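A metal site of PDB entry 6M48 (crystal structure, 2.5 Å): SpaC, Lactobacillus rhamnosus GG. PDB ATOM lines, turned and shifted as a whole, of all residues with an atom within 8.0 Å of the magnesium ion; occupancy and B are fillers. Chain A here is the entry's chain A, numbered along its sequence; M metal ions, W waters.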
ATOM      1  N   ASP A 115     -17.212 -18.630  -1.210  1.00  0.00           N
ATOM      2  CA  ASP A 115     -16.241 -19.503  -1.921  1.00  0.00           C
ATOM      3  C   ASP A 115     -14.843 -19.135  -1.417  1.00  0.00           C
ATOM      4  O   ASP A 115     -14.344 -18.070  -1.786  1.00  0.00           O
ATOM      5  CB  ASP A 115     -16.456 -19.313  -3.414  1.00  0.00           C
ATOM      6  CG  ASP A 115     -15.525 -20.078  -4.302  1.00  0.00           C
ATOM      7  OD1 ASP A 115     -14.426 -20.412  -3.783  1.00  0.00           O
ATOM      8  OD2 ASP A 115     -15.841 -20.210  -5.555  1.00  0.00           O
ATOM      9  N   MET A 116     -14.258 -19.980  -0.576  1.00  0.00           N
ATOM     10  CA  MET A 116     -12.894 -19.790  -0.025  1.00  0.00           C
ATOM     11  C   MET A 116     -11.969 -20.794  -0.697  1.00  0.00           C
ATOM     12  O   MET A 116     -10.966 -21.177  -0.063  1.00  0.00           O
ATOM     13  CB  MET A 116     -12.844 -19.977   1.496  1.00  0.00           C
ATOM     14  CG  MET A 116     -13.607 -18.920   2.236  1.00  0.00           C
ATOM     15  SD  MET A 116     -13.747 -19.392   3.988  1.00  0.00           S
ATOM     16  CE  MET A 116     -12.233 -18.743   4.685  1.00  0.00           C
ATOM     17  N   SER A 117     -12.332 -21.226  -1.911  1.00  0.00           N
ATOM     18  CA  SER A 117     -11.555 -22.151  -2.767  1.00  0.00           C
ATOM     19  C   SER A 117     -10.246 -21.500  -3.179  1.00  0.00           C
ATOM     20  O   SER A 117     -10.162 -20.265  -3.173  1.00  0.00           O
ATOM     21  CB  SER A 117     -12.334 -22.607  -3.985  1.00  0.00           C
ATOM     22  OG  SER A 117     -12.202 -21.701  -5.086  1.00  0.00           O
ATOM     23  N   GLY A 118      -9.266 -22.337  -3.541  1.00  0.00           N
ATOM     24  CA  GLY A 118      -7.961 -21.876  -4.024  1.00  0.00           C
ATOM     25  C   GLY A 118      -8.106 -21.160  -5.347  1.00  0.00           C
ATOM     26  O   GLY A 118      -7.431 -20.085  -5.477  1.00  0.00           O
ATOM     27  N   SER A 119      -9.012 -21.659  -6.232  1.00  0.00           N
ATOM     28  CA  SER A 119      -9.399 -21.046  -7.549  1.00  0.00           C
ATOM     29  C   SER A 119      -9.432 -19.517  -7.475  1.00  0.00           C
ATOM     30  O   SER A 119      -9.146 -18.893  -8.497  1.00  0.00           O
ATOM     31  CB  SER A 119     -10.753 -21.574  -8.073  1.00  0.00           C
ATOM     32  OG  SER A 119     -11.899 -20.875  -7.516  1.00  0.00           O
ATOM     33  N   MET A 120      -9.849 -18.965  -6.329  1.00  0.00           N
ATOM     34  CA  MET A 120     -10.051 -17.525  -6.071  1.00  0.00           C
ATOM     35  C   MET A 120      -8.747 -16.910  -5.572  1.00  0.00           C
ATOM     36  O   MET A 120      -8.831 -15.874  -4.827  1.00  0.00           O
ATOM     37  CB  MET A 120     -11.145 -17.337  -4.997  1.00  0.00           C
ATOM     38  CG  MET A 120     -12.575 -17.062  -5.543  1.00  0.00           C
ATOM     39  SD  MET A 120     -13.477 -15.779  -4.534  1.00  0.00           S
ATOM     40  CE  MET A 120     -12.368 -15.525  -3.147  1.00  0.00           C
ATOM     41  N   GLU A 121      -7.597 -17.496  -5.885  1.00  0.00           N
ATOM     42  CA  GLU A 121      -6.282 -16.855  -5.507  1.00  0.00           C
ATOM     43  C   GLU A 121      -5.167 -17.096  -6.553  1.00  0.00           C
ATOM     44  O   GLU A 121      -4.005 -16.858  -6.224  1.00  0.00           O
ATOM     45  CB  GLU A 121      -5.874 -17.181  -4.063  1.00  0.00           C
ATOM     46  CG  GLU A 121      -6.271 -16.076  -3.087  1.00  0.00           C
ATOM     47  CD  GLU A 121      -5.571 -16.218  -1.754  1.00  0.00           C
ATOM     48  OE1 GLU A 121      -4.483 -16.728  -1.812  1.00  0.00           O
ATOM     49  OE2 GLU A 121      -6.084 -15.826  -0.675  1.00  0.00           O
ATOM     50  N   ARG A 129      -8.892 -11.404  -4.677  1.00  0.00           N
ATOM     51  CA  ARG A 129     -10.357 -11.643  -4.575  1.00  0.00           C
ATOM     52  C   ARG A 129     -10.719 -11.809  -3.103  1.00  0.00           C
ATOM     53  O   ARG A 129     -11.659 -11.123  -2.641  1.00  0.00           O
ATOM     54  CB  ARG A 129     -10.791 -12.889  -5.336  1.00  0.00           C
ATOM     55  CG  ARG A 129     -10.508 -12.763  -6.801  1.00  0.00           C
ATOM     56  CD  ARG A 129     -11.166 -13.886  -7.543  1.00  0.00           C
ATOM     57  NE  ARG A 129     -10.698 -13.846  -8.924  1.00  0.00           N
ATOM     58  CZ  ARG A 129     -10.538 -14.891  -9.728  1.00  0.00           C
ATOM     59  NH1 ARG A 129     -10.837 -16.118  -9.327  1.00  0.00           N
ATOM     60  NH2 ARG A 129     -10.072 -14.711 -10.946  1.00  0.00           N
ATOM     61  N   PHE A 160     -16.768 -21.985   2.382  1.00  0.00           N
ATOM     62  CA  PHE A 160     -16.673 -23.364   1.896  1.00  0.00           C
ATOM     63  C   PHE A 160     -15.480 -23.506   0.950  1.00  0.00           C
ATOM     64  O   PHE A 160     -14.993 -22.532   0.356  1.00  0.00           O
ATOM     65  CB  PHE A 160     -17.982 -23.733   1.239  1.00  0.00           C
ATOM     66  CG  PHE A 160     -18.229 -23.054  -0.081  1.00  0.00           C
ATOM     67  CD1 PHE A 160     -17.740 -23.592  -1.257  1.00  0.00           C
ATOM     68  CD2 PHE A 160     -18.992 -21.901  -0.133  1.00  0.00           C
ATOM     69  CE1 PHE A 160     -18.019 -22.977  -2.472  1.00  0.00           C
ATOM     70  CE2 PHE A 160     -19.290 -21.302  -1.348  1.00  0.00           C
ATOM     71  CZ  PHE A 160     -18.775 -21.832  -2.513  1.00  0.00           C
ATOM     72  N   SER A 161     -15.047 -24.763   0.877  1.00  0.00           N
ATOM     73  CA  SER A 161     -13.867 -25.253   0.133  1.00  0.00           C
ATOM     74  C   SER A 161     -14.206 -26.685  -0.309  1.00  0.00           C
ATOM     75  O   SER A 161     -15.205 -26.828  -0.965  1.00  0.00           O
ATOM     76  CB  SER A 161     -12.694 -25.194   1.030  1.00  0.00           C
ATOM     77  OG  SER A 161     -11.643 -24.725   0.288  1.00  0.00           O
ATOM     78  N   GLN A 198      -8.143 -21.560   0.418  1.00  0.00           N
ATOM     79  CA  GLN A 198      -7.506 -22.740  -0.233  1.00  0.00           C
ATOM     80  C   GLN A 198      -8.566 -23.832  -0.373  1.00  0.00           C
ATOM     81  O   GLN A 198      -9.340 -23.982   0.546  1.00  0.00           O
ATOM     82  CB  GLN A 198      -6.308 -23.273   0.585  1.00  0.00           C
ATOM     83  CG  GLN A 198      -6.550 -23.424   2.085  1.00  0.00           C
ATOM     84  CD  GLN A 198      -6.279 -24.830   2.604  1.00  0.00           C
ATOM     85  OE1 GLN A 198      -5.262 -25.435   2.257  1.00  0.00           O
ATOM     86  NE2 GLN A 198      -7.185 -25.375   3.420  1.00  0.00           N
ATOM     87  N   GLY A 199      -8.514 -24.602  -1.437  1.00  0.00           N
ATOM     88  CA  GLY A 199      -9.264 -25.844  -1.588  1.00  0.00           C
ATOM     89  C   GLY A 199     -10.111 -25.864  -2.846  1.00  0.00           C
ATOM     90  O   GLY A 199      -9.960 -24.909  -3.672  1.00  0.00           O
ATOM     91  N   GLY A 200     -10.936 -26.915  -2.985  1.00  0.00           N
ATOM     92  CA  GLY A 200     -11.943 -27.062  -4.053  1.00  0.00           C
ATOM     93  C   GLY A 200     -13.148 -26.141  -3.848  1.00  0.00           C
ATOM     94  O   GLY A 200     -13.074 -25.294  -2.972  1.00  0.00           O
ATOM     95  N   THR A 201     -14.232 -26.353  -4.608  1.00  0.00           N
ATOM     96  CA  THR A 201     -15.458 -25.517  -4.648  1.00  0.00           C
ATOM     97  C   THR A 201     -16.669 -26.429  -4.459  1.00  0.00           C
ATOM     98  O   THR A 201     -17.231 -26.905  -5.434  1.00  0.00           O
ATOM     99  CB  THR A 201     -15.500 -24.696  -5.938  1.00  0.00           C
ATOM    100  OG1 THR A 201     -14.233 -24.075  -6.206  1.00  0.00           O
ATOM    101  CG2 THR A 201     -16.539 -23.604  -5.915  1.00  0.00           C
ATOM    102  N   TYR A 202     -17.084 -26.645  -3.218  1.00  0.00           N
ATOM    103  CA  TYR A 202     -18.283 -27.407  -2.829  1.00  0.00           C
ATOM    104  C   TYR A 202     -19.415 -26.401  -2.673  1.00  0.00           C
ATOM    105  O   TYR A 202     -19.990 -26.303  -1.562  1.00  0.00           O
ATOM    106  CB  TYR A 202     -17.958 -28.177  -1.548  1.00  0.00           C
ATOM    107  CG  TYR A 202     -18.888 -29.286  -1.151  1.00  0.00           C
ATOM    108  CD1 TYR A 202     -19.864 -29.775  -1.990  1.00  0.00           C
ATOM    109  CD2 TYR A 202     -18.734 -29.876   0.094  1.00  0.00           C
ATOM    110  CE1 TYR A 202     -20.666 -30.828  -1.577  1.00  0.00           C
ATOM    111  CE2 TYR A 202     -19.509 -30.942   0.511  1.00  0.00           C
ATOM    112  CZ  TYR A 202     -20.490 -31.412  -0.331  1.00  0.00           C
ATOM    113  OH  TYR A 202     -21.320 -32.418   0.091  1.00  0.00           O
ATOM    114  N   THR A 203     -19.759 -25.712  -3.773  1.00  0.00           N
ATOM    115  CA  THR A 203     -20.833 -24.687  -3.786  1.00  0.00           C
ATOM    116  C   THR A 203     -22.099 -25.249  -3.149  1.00  0.00           C
ATOM    117  O   THR A 203     -22.742 -24.548  -2.341  1.00  0.00           O
ATOM    118  CB  THR A 203     -21.102 -24.163  -5.201  1.00  0.00           C
ATOM    119  OG1 THR A 203     -19.849 -23.792  -5.773  1.00  0.00           O
ATOM    120  CG2 THR A 203     -22.064 -22.998  -5.171  1.00  0.00           C
ATOM    121  N   THR A 229     -18.541 -16.073  -5.356  1.00  0.00           N
ATOM    122  CA  THR A 229     -17.769 -17.219  -5.880  1.00  0.00           C
ATOM    123  C   THR A 229     -17.170 -16.879  -7.232  1.00  0.00           C
ATOM    124  O   THR A 229     -17.719 -15.974  -7.882  1.00  0.00           O
ATOM    125  CB  THR A 229     -18.703 -18.422  -6.006  1.00  0.00           C
ATOM    126  OG1 THR A 229     -18.067 -19.542  -6.606  1.00  0.00           O
ATOM    127  CG2 THR A 229     -19.900 -18.060  -6.847  1.00  0.00           C
ATOM    128  N   ASP A 230     -16.187 -17.650  -7.710  1.00  0.00           N
ATOM    129  CA  ASP A 230     -15.777 -17.453  -9.131  1.00  0.00           C
ATOM    130  C   ASP A 230     -16.629 -18.292 -10.070  1.00  0.00           C
ATOM    131  O   ASP A 230     -16.635 -17.963 -11.293  1.00  0.00           O
ATOM    132  CB  ASP A 230     -14.308 -17.623  -9.384  1.00  0.00           C
ATOM    133  CG  ASP A 230     -13.772 -18.929  -8.868  1.00  0.00           C
ATOM    134  OD1 ASP A 230     -14.087 -19.976  -9.494  1.00  0.00           O
ATOM    135  OD2 ASP A 230     -13.099 -18.850  -7.812  1.00  0.00           O
ATOM    136  N   GLY A 231     -17.393 -19.255  -9.552  1.00  0.00           N
ATOM    137  CA  GLY A 231     -18.559 -19.788 -10.287  1.00  0.00           C
ATOM    138  C   GLY A 231     -18.470 -21.258 -10.617  1.00  0.00           C
ATOM    139  O   GLY A 231     -19.505 -21.771 -11.110  1.00  0.00           O
ATOM    140  N   VAL A 232     -17.332 -21.952 -10.459  1.00  0.00           N
ATOM    141  CA  VAL A 232     -17.406 -23.357 -10.964  1.00  0.00           C
ATOM    142  C   VAL A 232     -17.326 -24.336  -9.813  1.00  0.00           C
ATOM    143  O   VAL A 232     -16.260 -24.582  -9.281  1.00  0.00           O
ATOM    144  CB  VAL A 232     -16.417 -23.603 -12.104  1.00  0.00           C
ATOM    145  CG1 VAL A 232     -16.037 -25.068 -12.214  1.00  0.00           C
ATOM    146  CG2 VAL A 232     -17.044 -23.110 -13.389  1.00  0.00           C
ATOM    147  N   PRO A 233     -18.435 -24.957  -9.406  1.00  0.00           N
ATOM    148  CA  PRO A 233     -18.418 -26.008  -8.411  1.00  0.00           C
ATOM    149  C   PRO A 233     -17.622 -27.229  -8.913  1.00  0.00           C
ATOM    150  O   PRO A 233     -17.794 -27.630 -10.053  1.00  0.00           O
ATOM    151  CB  PRO A 233     -19.887 -26.430  -8.271  1.00  0.00           C
ATOM    152  CG  PRO A 233     -20.657 -25.349  -8.895  1.00  0.00           C
ATOM    153  CD  PRO A 233     -19.769 -24.788  -9.983  1.00  0.00           C
ATOM    154  N   THR A 234     -16.732 -27.757  -8.091  1.00  0.00           N
ATOM    155  CA  THR A 234     -15.915 -28.945  -8.423  1.00  0.00           C
ATOM    156  C   THR A 234     -16.240 -30.081  -7.466  1.00  0.00           C
ATOM    157  O   THR A 234     -15.619 -31.143  -7.603  1.00  0.00           O
ATOM    158  CB  THR A 234     -14.451 -28.543  -8.479  1.00  0.00           C
ATOM    159  OG1 THR A 234     -14.180 -27.952  -7.227  1.00  0.00           O
ATOM    160  CG2 THR A 234     -14.164 -27.557  -9.594  1.00  0.00           C
ATOM    161  N   GLY A 262     -13.024 -31.944  -9.005  1.00  0.00           N
ATOM    162  CA  GLY A 262     -11.887 -31.283  -8.335  1.00  0.00           C
ATOM    163  C   GLY A 262     -11.440 -29.993  -8.982  1.00  0.00           C
ATOM    164  O   GLY A 262     -11.401 -29.013  -8.258  1.00  0.00           O
ATOM    165  N   ASN A 263     -11.095 -29.982 -10.277  1.00  0.00           N
ATOM    166  CA  ASN A 263     -10.541 -28.799 -10.981  1.00  0.00           C
ATOM    167  C   ASN A 263     -11.437 -28.413 -12.171  1.00  0.00           C
ATOM    168  O   ASN A 263     -11.030 -27.580 -12.995  1.00  0.00           O
ATOM    169  CB  ASN A 263      -9.098 -29.028 -11.429  1.00  0.00           C
ATOM    170  CG  ASN A 263      -8.855 -30.344 -12.161  1.00  0.00           C
ATOM    171  OD1 ASN A 263      -9.755 -30.992 -12.736  1.00  0.00           O
ATOM    172  ND2 ASN A 263      -7.578 -30.723 -12.157  1.00  0.00           N
HETATM  173 MG    MG M   1     -12.879 -22.610  -6.896  1.00  0.00          MG
HETATM  174  O   HOH W   1     -14.579 -21.349  -7.108  1.00  0.00           O
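Water W1 lies within hydrogen-bond range of the side-chain carboxylate (OD1) of Asp 230 and the side-chain carboxylate (OD1) of Asp 115.
The backbone carbonyl oxygen (O) of Ser 119 sits at hydrogen-bond distance from the guanidinium group (NH1) of Arg 129 (3.4 Å).
N of Asp 230 sits at hydrogen-bond distance from OD2 of Asp 115.
OD2 of Asp 230 lies within salt-bridge range of NH1 of Arg 129, at 3.9 Å.
The backbone NH (N) of Ser 117 sits at hydrogen-bond distance from the side-chain carboxylate (OD1) of Asp 115, 2.9 Å away.
The backbone NH of Thr 234 sits at hydrogen-bond distance from the backbone carbonyl oxygen of Thr 201 (2.8 Å).
The side-chain hydroxyl (OG) of Ser 119 sits close to the side-chain carboxylate (OD1) of Asp 230 (3.1 Å).
The magnesium ion is bound by the side-chain hydroxyl of Ser 119 (2.1 Å), the side-chain hydroxyl of Thr 201 (2.1 Å), water W1 (2.1 Å) and the side-chain hydroxyl of Ser 117 (2.1 Å).
The magnesium ion has four donor atoms within binding distance.
Merely in contact with the magnesium ion: Asp 230 (3.9 Å).
Along chain A the residues within 4 Å of the magnesium ion span positions 117 to 230.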
